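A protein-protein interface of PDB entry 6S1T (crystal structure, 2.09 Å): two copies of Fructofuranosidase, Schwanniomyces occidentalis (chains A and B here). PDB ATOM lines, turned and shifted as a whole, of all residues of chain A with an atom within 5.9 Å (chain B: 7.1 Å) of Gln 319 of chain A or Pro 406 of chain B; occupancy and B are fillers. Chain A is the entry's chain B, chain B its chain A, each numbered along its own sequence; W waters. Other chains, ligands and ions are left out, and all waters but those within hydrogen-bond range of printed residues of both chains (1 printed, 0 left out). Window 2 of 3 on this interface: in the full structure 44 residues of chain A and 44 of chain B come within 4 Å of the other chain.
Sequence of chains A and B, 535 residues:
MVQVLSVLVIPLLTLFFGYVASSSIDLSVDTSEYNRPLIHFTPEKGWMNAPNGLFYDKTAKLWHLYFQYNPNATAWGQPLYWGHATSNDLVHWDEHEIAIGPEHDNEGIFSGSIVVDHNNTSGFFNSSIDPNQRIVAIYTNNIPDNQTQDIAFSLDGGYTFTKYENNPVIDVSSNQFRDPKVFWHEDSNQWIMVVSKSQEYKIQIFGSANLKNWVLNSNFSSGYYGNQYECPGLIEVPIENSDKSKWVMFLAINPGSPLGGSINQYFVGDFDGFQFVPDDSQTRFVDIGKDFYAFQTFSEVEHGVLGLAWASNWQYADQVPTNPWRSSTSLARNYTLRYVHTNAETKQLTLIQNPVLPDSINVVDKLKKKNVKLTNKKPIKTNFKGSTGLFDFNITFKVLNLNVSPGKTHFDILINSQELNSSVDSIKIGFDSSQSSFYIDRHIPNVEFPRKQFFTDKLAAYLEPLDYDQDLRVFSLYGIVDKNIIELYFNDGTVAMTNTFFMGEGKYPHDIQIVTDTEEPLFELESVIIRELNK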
ATOM      1  N   TRP A  47       2.678  21.474  -0.724  1.00  0.00           N
ATOM      2  CA  TRP A  47       1.427  20.672  -0.613  1.00  0.00           C
ATOM      3  C   TRP A  47       0.529  20.943  -1.822  1.00  0.00           C
ATOM      4  O   TRP A  47       0.382  22.112  -2.202  1.00  0.00           O
ATOM      5  CB  TRP A  47       0.711  20.996   0.697  1.00  0.00           C
ATOM      6  CG  TRP A  47      -0.730  20.588   0.722  1.00  0.00           C
ATOM      7  CD1 TRP A  47      -1.805  21.343   0.357  1.00  0.00           C
ATOM      8  CD2 TRP A  47      -1.253  19.318   1.139  1.00  0.00           C
ATOM      9  NE1 TRP A  47      -2.961  20.632   0.528  1.00  0.00           N
ATOM     10  CE2 TRP A  47      -2.655  19.385   1.000  1.00  0.00           C
ATOM     11  CE3 TRP A  47      -0.680  18.135   1.612  1.00  0.00           C
ATOM     12  CZ2 TRP A  47      -3.486  18.313   1.307  1.00  0.00           C
ATOM     13  CZ3 TRP A  47      -1.503  17.066   1.892  1.00  0.00           C
ATOM     14  CH2 TRP A  47      -2.888  17.165   1.761  1.00  0.00           C
ATOM     15  N   THR A  74       4.270  20.895   3.670  1.00  0.00           N
ATOM     16  CA  THR A  74       3.708  19.640   3.100  1.00  0.00           C
ATOM     17  C   THR A  74       2.396  19.306   3.820  1.00  0.00           C
ATOM     18  O   THR A  74       2.144  18.123   4.092  1.00  0.00           O
ATOM     19  CB  THR A  74       4.738  18.503   3.090  1.00  0.00           C
ATOM     20  OG1 THR A  74       5.372  18.391   4.368  1.00  0.00           O
ATOM     21  CG2 THR A  74       5.751  18.700   1.981  1.00  0.00           C
ATOM     22  N   GLN A 315      -8.391  11.954   4.919  1.00  0.00           N
ATOM     23  CA  GLN A 315      -8.170  11.308   6.236  1.00  0.00           C
ATOM     24  C   GLN A 315      -6.677  11.286   6.571  1.00  0.00           C
ATOM     25  O   GLN A 315      -6.363  11.431   7.760  1.00  0.00           O
ATOM     26  CB  GLN A 315      -8.718   9.888   6.273  1.00  0.00           C
ATOM     27  CG  GLN A 315     -10.234   9.802   6.275  1.00  0.00           C
ATOM     28  CD  GLN A 315     -10.670   8.357   6.202  1.00  0.00           C
ATOM     29  OE1 GLN A 315     -10.129   7.563   5.427  1.00  0.00           O
ATOM     30  NE2 GLN A 315     -11.634   7.999   7.045  1.00  0.00           N
ATOM     31  N   TYR A 316      -5.800  11.048   5.589  1.00  0.00           N
ATOM     32  CA  TYR A 316      -4.354  10.788   5.833  1.00  0.00           C
ATOM     33  C   TYR A 316      -3.439  11.529   4.842  1.00  0.00           C
ATOM     34  O   TYR A 316      -2.218  11.386   4.977  1.00  0.00           O
ATOM     35  CB  TYR A 316      -4.077   9.282   5.778  1.00  0.00           C
ATOM     36  CG  TYR A 316      -4.675   8.545   4.602  1.00  0.00           C
ATOM     37  CD1 TYR A 316      -4.135   8.658   3.326  1.00  0.00           C
ATOM     38  CD2 TYR A 316      -5.775   7.712   4.763  1.00  0.00           C
ATOM     39  CE1 TYR A 316      -4.676   7.972   2.247  1.00  0.00           C
ATOM     40  CE2 TYR A 316      -6.336   7.035   3.687  1.00  0.00           C
ATOM     41  CZ  TYR A 316      -5.792   7.169   2.420  1.00  0.00           C
ATOM     42  OH  TYR A 316      -6.323   6.484   1.355  1.00  0.00           O
ATOM     43  N   ALA A 317      -3.978  12.294   3.890  1.00  0.00           N
ATOM     44  CA  ALA A 317      -3.188  12.889   2.787  1.00  0.00           C
ATOM     45  C   ALA A 317      -1.973  13.662   3.331  1.00  0.00           C
ATOM     46  O   ALA A 317      -0.898  13.599   2.693  1.00  0.00           O
ATOM     47  CB  ALA A 317      -4.060  13.776   1.938  1.00  0.00           C
ATOM     48  N   ASP A 318      -2.122  14.391   4.438  1.00  0.00           N
ATOM     49  CA  ASP A 318      -1.053  15.314   4.920  1.00  0.00           C
ATOM     50  C   ASP A 318      -0.068  14.581   5.843  1.00  0.00           C
ATOM     51  O   ASP A 318       0.786  15.270   6.412  1.00  0.00           O
ATOM     52  CB  ASP A 318      -1.629  16.583   5.545  1.00  0.00           C
ATOM     53  CG  ASP A 318      -2.380  16.386   6.845  1.00  0.00           C
ATOM     54  OD1 ASP A 318      -2.414  15.244   7.348  1.00  0.00           O
ATOM     55  OD2 ASP A 318      -2.974  17.369   7.306  1.00  0.00           O
ATOM     56  N   GLN A 319      -0.141  13.245   5.930  1.00  0.00           N
ATOM     57  CA  GLN A 319       0.710  12.446   6.850  1.00  0.00           C
ATOM     58  C   GLN A 319       1.545  11.396   6.107  1.00  0.00           C
ATOM     59  O   GLN A 319       2.369  10.759   6.775  1.00  0.00           O
ATOM     60  CB  GLN A 319      -0.144  11.763   7.920  1.00  0.00           C
ATOM     61  CG  GLN A 319      -0.964  12.753   8.726  1.00  0.00           C
ATOM     62  CD  GLN A 319      -0.085  13.712   9.488  1.00  0.00           C
ATOM     63  OE1 GLN A 319       0.978  13.336   9.989  1.00  0.00           O
ATOM     64  NE2 GLN A 319      -0.522  14.952   9.582  1.00  0.00           N
ATOM     65  N   VAL A 320       1.334  11.181   4.811  1.00  0.00           N
ATOM     66  CA  VAL A 320       2.002  10.066   4.079  1.00  0.00           C
ATOM     67  C   VAL A 320       3.495  10.390   3.969  1.00  0.00           C
ATOM     68  O   VAL A 320       3.885  11.557   3.920  1.00  0.00           O
ATOM     69  CB  VAL A 320       1.358   9.814   2.701  1.00  0.00           C
ATOM     70  CG1 VAL A 320      -0.094   9.359   2.828  1.00  0.00           C
ATOM     71  CG2 VAL A 320       1.466  11.025   1.788  1.00  0.00           C
ATOM     72  N   PRO A 321       4.373   9.363   3.940  1.00  0.00           N
ATOM     73  CA  PRO A 321       5.819   9.582   3.969  1.00  0.00           C
ATOM     74  C   PRO A 321       6.438   9.934   2.611  1.00  0.00           C
ATOM     75  O   PRO A 321       7.278   9.199   2.102  1.00  0.00           O
ATOM     76  CB  PRO A 321       6.336   8.243   4.494  1.00  0.00           C
ATOM     77  CG  PRO A 321       5.357   7.244   3.917  1.00  0.00           C
ATOM     78  CD  PRO A 321       4.012   7.937   3.991  1.00  0.00           C
ATOM     79  N   ARG A 326       3.850  16.664  -0.976  1.00  0.00           N
ATOM     80  CA  ARG A 326       2.779  15.646  -0.780  1.00  0.00           C
ATOM     81  C   ARG A 326       1.729  15.812  -1.876  1.00  0.00           C
ATOM     82  O   ARG A 326       1.387  16.964  -2.181  1.00  0.00           O
ATOM     83  CB  ARG A 326       2.150  15.746   0.610  1.00  0.00           C
ATOM     84  CG  ARG A 326       2.954  15.069   1.707  1.00  0.00           C
ATOM     85  CD  ARG A 326       2.186  14.985   3.014  1.00  0.00           C
ATOM     86  NE  ARG A 326       2.929  14.198   3.985  1.00  0.00           N
ATOM     87  CZ  ARG A 326       3.607  14.693   5.016  1.00  0.00           C
ATOM     88  NH1 ARG A 326       3.602  15.990   5.271  1.00  0.00           N
ATOM     89  NH2 ARG A 326       4.267  13.865   5.811  1.00  0.00           N
ATOM     90  N   PHE A 449       2.734   5.738   9.809  1.00  0.00           N
ATOM     91  CA  PHE A 449       2.541   7.205   9.721  1.00  0.00           C
ATOM     92  C   PHE A 449       1.261   7.560  10.464  1.00  0.00           C
ATOM     93  O   PHE A 449       0.363   6.728  10.602  1.00  0.00           O
ATOM     94  CB  PHE A 449       2.599   7.681   8.266  1.00  0.00           C
ATOM     95  CG  PHE A 449       1.673   6.992   7.294  1.00  0.00           C
ATOM     96  CD1 PHE A 449       0.376   7.445   7.118  1.00  0.00           C
ATOM     97  CD2 PHE A 449       2.109   5.929   6.523  1.00  0.00           C
ATOM     98  CE1 PHE A 449      -0.471   6.838   6.204  1.00  0.00           C
ATOM     99  CE2 PHE A 449       1.267   5.329   5.600  1.00  0.00           C
ATOM    100  CZ  PHE A 449      -0.024   5.775   5.454  1.00  0.00           C
ATOM    101  N   PRO A 450       1.158   8.798  10.990  1.00  0.00           N
ATOM    102  CA  PRO A 450      -0.047   9.243  11.686  1.00  0.00           C
ATOM    103  C   PRO A 450      -1.321   9.014  10.855  1.00  0.00           C
ATOM    104  O   PRO A 450      -1.278   9.213   9.648  1.00  0.00           O
ATOM    105  CB  PRO A 450       0.204  10.741  11.882  1.00  0.00           C
ATOM    106  CG  PRO A 450       1.712  10.853  11.951  1.00  0.00           C
ATOM    107  CD  PRO A 450       2.204   9.832  10.948  1.00  0.00           C
ATOM    108  N   ARG A 451      -2.401   8.594  11.526  1.00  0.00           N
ATOM    109  CA  ARG A 451      -3.761   8.342  10.964  1.00  0.00           C
ATOM    110  C   ARG A 451      -3.738   7.163   9.970  1.00  0.00           C
ATOM    111  O   ARG A 451      -4.620   7.113   9.093  1.00  0.00           O
ATOM    112  CB  ARG A 451      -4.345   9.640  10.386  1.00  0.00           C
ATOM    113  CG  ARG A 451      -4.157  10.823  11.329  1.00  0.00           C
ATOM    114  CD  ARG A 451      -5.222  11.884  11.260  1.00  0.00           C
ATOM    115  NE  ARG A 451      -5.218  12.521   9.957  1.00  0.00           N
ATOM    116  CZ  ARG A 451      -4.608  13.664   9.662  1.00  0.00           C
ATOM    117  NH1 ARG A 451      -3.928  14.334  10.588  1.00  0.00           N
ATOM    118  NH2 ARG A 451      -4.695  14.130   8.427  1.00  0.00           N
ATOM    119  N   VAL B 404      -1.486  18.651  20.078  1.00  0.00           N
ATOM    120  CA  VAL B 404      -0.553  17.495  20.186  1.00  0.00           C
ATOM    121  C   VAL B 404      -0.098  17.180  18.767  1.00  0.00           C
ATOM    122  O   VAL B 404      -0.804  17.608  17.821  1.00  0.00           O
ATOM    123  CB  VAL B 404      -1.251  16.311  20.879  1.00  0.00           C
ATOM    124  CG1 VAL B 404      -1.751  16.714  22.266  1.00  0.00           C
ATOM    125  CG2 VAL B 404      -2.393  15.768  20.032  1.00  0.00           C
ATOM    126  N   SER B 405       1.025  16.481  18.619  1.00  0.00           N
ATOM    127  CA  SER B 405       1.555  16.066  17.294  1.00  0.00           C
ATOM    128  C   SER B 405       0.542  15.140  16.619  1.00  0.00           C
ATOM    129  O   SER B 405      -0.217  14.455  17.302  1.00  0.00           O
ATOM    130  CB  SER B 405       2.899  15.412  17.432  1.00  0.00           C
ATOM    131  OG  SER B 405       2.815  14.283  18.282  1.00  0.00           O
ATOM    132  N   PRO B 406       0.506  15.096  15.263  1.00  0.00           N
ATOM    133  CA  PRO B 406      -0.582  14.449  14.524  1.00  0.00           C
ATOM    134  C   PRO B 406      -0.774  12.948  14.797  1.00  0.00           C
ATOM    135  O   PRO B 406      -1.874  12.478  14.634  1.00  0.00           O
ATOM    136  CB  PRO B 406      -0.229  14.697  13.044  1.00  0.00           C
ATOM    137  CG  PRO B 406       1.243  15.033  13.046  1.00  0.00           C
ATOM    138  CD  PRO B 406       1.498  15.718  14.369  1.00  0.00           C
ATOM    139  N   GLY B 407       0.270  12.246  15.241  1.00  0.00           N
ATOM    140  CA  GLY B 407       0.206  10.806  15.551  1.00  0.00           C
ATOM    141  C   GLY B 407      -0.492  10.511  16.878  1.00  0.00           C
ATOM    142  O   GLY B 407      -0.692   9.311  17.186  1.00  0.00           O
ATOM    143  N   LYS B 408      -0.862  11.545  17.635  1.00  0.00           N
ATOM    144  CA  LYS B 408      -1.320  11.396  19.041  1.00  0.00           C
ATOM    145  C   LYS B 408      -2.716  11.978  19.258  1.00  0.00           C
ATOM    146  O   LYS B 408      -3.161  11.972  20.409  1.00  0.00           O
ATOM    147  CB  LYS B 408      -0.297  12.050  19.969  1.00  0.00           C
ATOM    148  CG  LYS B 408       1.032  11.315  20.029  1.00  0.00           C
ATOM    149  CD  LYS B 408       2.046  12.050  20.847  1.00  0.00           C
ATOM    150  CE  LYS B 408       3.249  11.205  21.180  1.00  0.00           C
ATOM    151  NZ  LYS B 408       3.991  11.824  22.300  1.00  0.00           N
ATOM    152  N   THR B 409      -3.399  12.425  18.203  1.00  0.00           N
ATOM    153  CA  THR B 409      -4.756  13.023  18.294  1.00  0.00           C
ATOM    154  C   THR B 409      -5.826  11.930  18.421  1.00  0.00           C
ATOM    155  O   THR B 409      -6.846  12.021  17.696  1.00  0.00           O
ATOM    156  CB  THR B 409      -5.045  13.920  17.083  1.00  0.00           C
ATOM    157  OG1 THR B 409      -4.997  13.134  15.888  1.00  0.00           O
ATOM    158  CG2 THR B 409      -4.093  15.099  17.022  1.00  0.00           C
ATOM    159  N   HIS B 410      -5.621  10.935  19.282  1.00  0.00           N
ATOM    160  CA  HIS B 410      -6.563   9.792  19.407  1.00  0.00           C
ATOM    161  C   HIS B 410      -6.365   8.997  20.700  1.00  0.00           C
ATOM    162  O   HIS B 410      -5.305   9.105  21.347  1.00  0.00           O
ATOM    163  CB  HIS B 410      -6.415   8.847  18.218  1.00  0.00           C
ATOM    164  CG  HIS B 410      -5.097   8.158  18.187  1.00  0.00           C
ATOM    165  ND1 HIS B 410      -4.910   6.893  18.709  1.00  0.00           N
ATOM    166  CD2 HIS B 410      -3.891   8.562  17.736  1.00  0.00           C
ATOM    167  CE1 HIS B 410      -3.651   6.537  18.560  1.00  0.00           C
ATOM    168  NE2 HIS B 410      -3.000   7.544  17.971  1.00  0.00           N
ATOM    169  N   ASP B 432     -10.365   9.525  16.707  1.00  0.00           N
ATOM    170  CA  ASP B 432      -9.375  10.567  16.337  1.00  0.00           C
ATOM    171  C   ASP B 432     -10.068  11.932  16.343  1.00  0.00           C
ATOM    172  O   ASP B 432     -11.010  12.126  15.543  1.00  0.00           O
ATOM    173  CB  ASP B 432      -8.724  10.266  14.986  1.00  0.00           C
ATOM    174  CG  ASP B 432      -7.497  11.132  14.732  1.00  0.00           C
ATOM    175  OD1 ASP B 432      -7.664  12.367  14.610  1.00  0.00           O
ATOM    176  OD2 ASP B 432      -6.378  10.572  14.696  1.00  0.00           O
ATOM    177  N   SER B 434      -8.814  14.901  15.386  1.00  0.00           N
ATOM    178  CA  SER B 434      -8.548  15.663  14.130  1.00  0.00           C
ATOM    179  C   SER B 434      -9.576  15.263  13.052  1.00  0.00           C
ATOM    180  O   SER B 434      -9.957  16.138  12.269  1.00  0.00           O
ATOM    181  CB  SER B 434      -7.119  15.514  13.638  1.00  0.00           C
ATOM    182  OG  SER B 434      -6.877  14.213  13.091  1.00  0.00           O
HETATM  183  O   HOH W   1      -3.813  14.206  13.443  1.00  0.00           O
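Water W1 lies within hydrogen-bond range of O of Pro 406 of chain B (2.9 Å), NH1 of Arg 451 of chain A (2.9 Å), OG1 of Thr 409 of chain B (2.9 Å) and OG of Ser 434 of chain B (3.1 Å).
Gln 319 of chain A touches Pro 406 of chain B (NE2 to CB, 3.5 Å).
Pro 450 of chain A touches Pro 406 of chain B (CB to C, 3.8 Å).
CB of Pro 450 of chain A touches CA of Gly 407 of chain B (3.7 Å).
OD2 of Asp 432 of chain B touches CD of Arg 451 of chain A (3.9 Å).
Arg 451 of chain A touches Ser 434 of chain B.
Of chain B, only Pro 406 comes within 4 Å of Gln 319 of chain A.
Pro 406 of chain B touches just these residues of chain A: Gln 319 (3.5 Å) and Pro 450 (3.8 Å).
Of the printed residues of chain B, Pro 450 of chain A touches Pro 406 (3.8 Å) and Gly 407 (3.7 Å).
Of the printed residues of chain A, Gly 407 of chain B touches Pro 450.
Printed residues of chain B within 4 Å of Arg 451 of chain A: Asp 432 (3.9 Å) and Ser 434 (3.4 Å).
Gln 315 of chain A touches none of the printed residues of chain B.
Ser 405 of chain B touches none of the printed residues of chain A.
The nearest residue of chain B that does not touch Gln 319 of chain A is Gly 407 of chain B (5.4 Å).
No position is printed for both chains.
Of the 5 pairs that touch across the chains among the printed residues, none has its exchanged pair printed and touching as well.
OG1 of Thr 409 of chain B is in hydrogen-bond range of OD1 of Asp 432 of chain B (3.1 Å).
OG1 of Thr 409 of chain B lies within hydrogen-bond range of O of Pro 406 of chain B.
The backbone carbonyl oxygen (O) of Gln 315 of chain A sits at hydrogen-bond distance from the guanidinium group (NE) of Arg 451 of chain A, 2.7 Å away.
The side-chain hydroxyl (OG) of Ser 434 of chain B is in hydrogen-bond range of the side-chain carboxylate (OD1) of Asp 432 of chain B (2.5 Å).
A ring nitrogen (NE2) of His 410 of chain B sits at hydrogen-bond distance from the backbone carbonyl oxygen (O) of Gly 407 of chain B, 3.0 Å away.
The side-chain amide nitrogen of Gln 319 of chain A is in hydrogen-bond range of the side-chain carboxylate of Asp 318 of chain A (2.9 Å).
Hydrophobic or aromatic side chains of chain B within 4 Å of the printed part of chain A: Pro 406.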
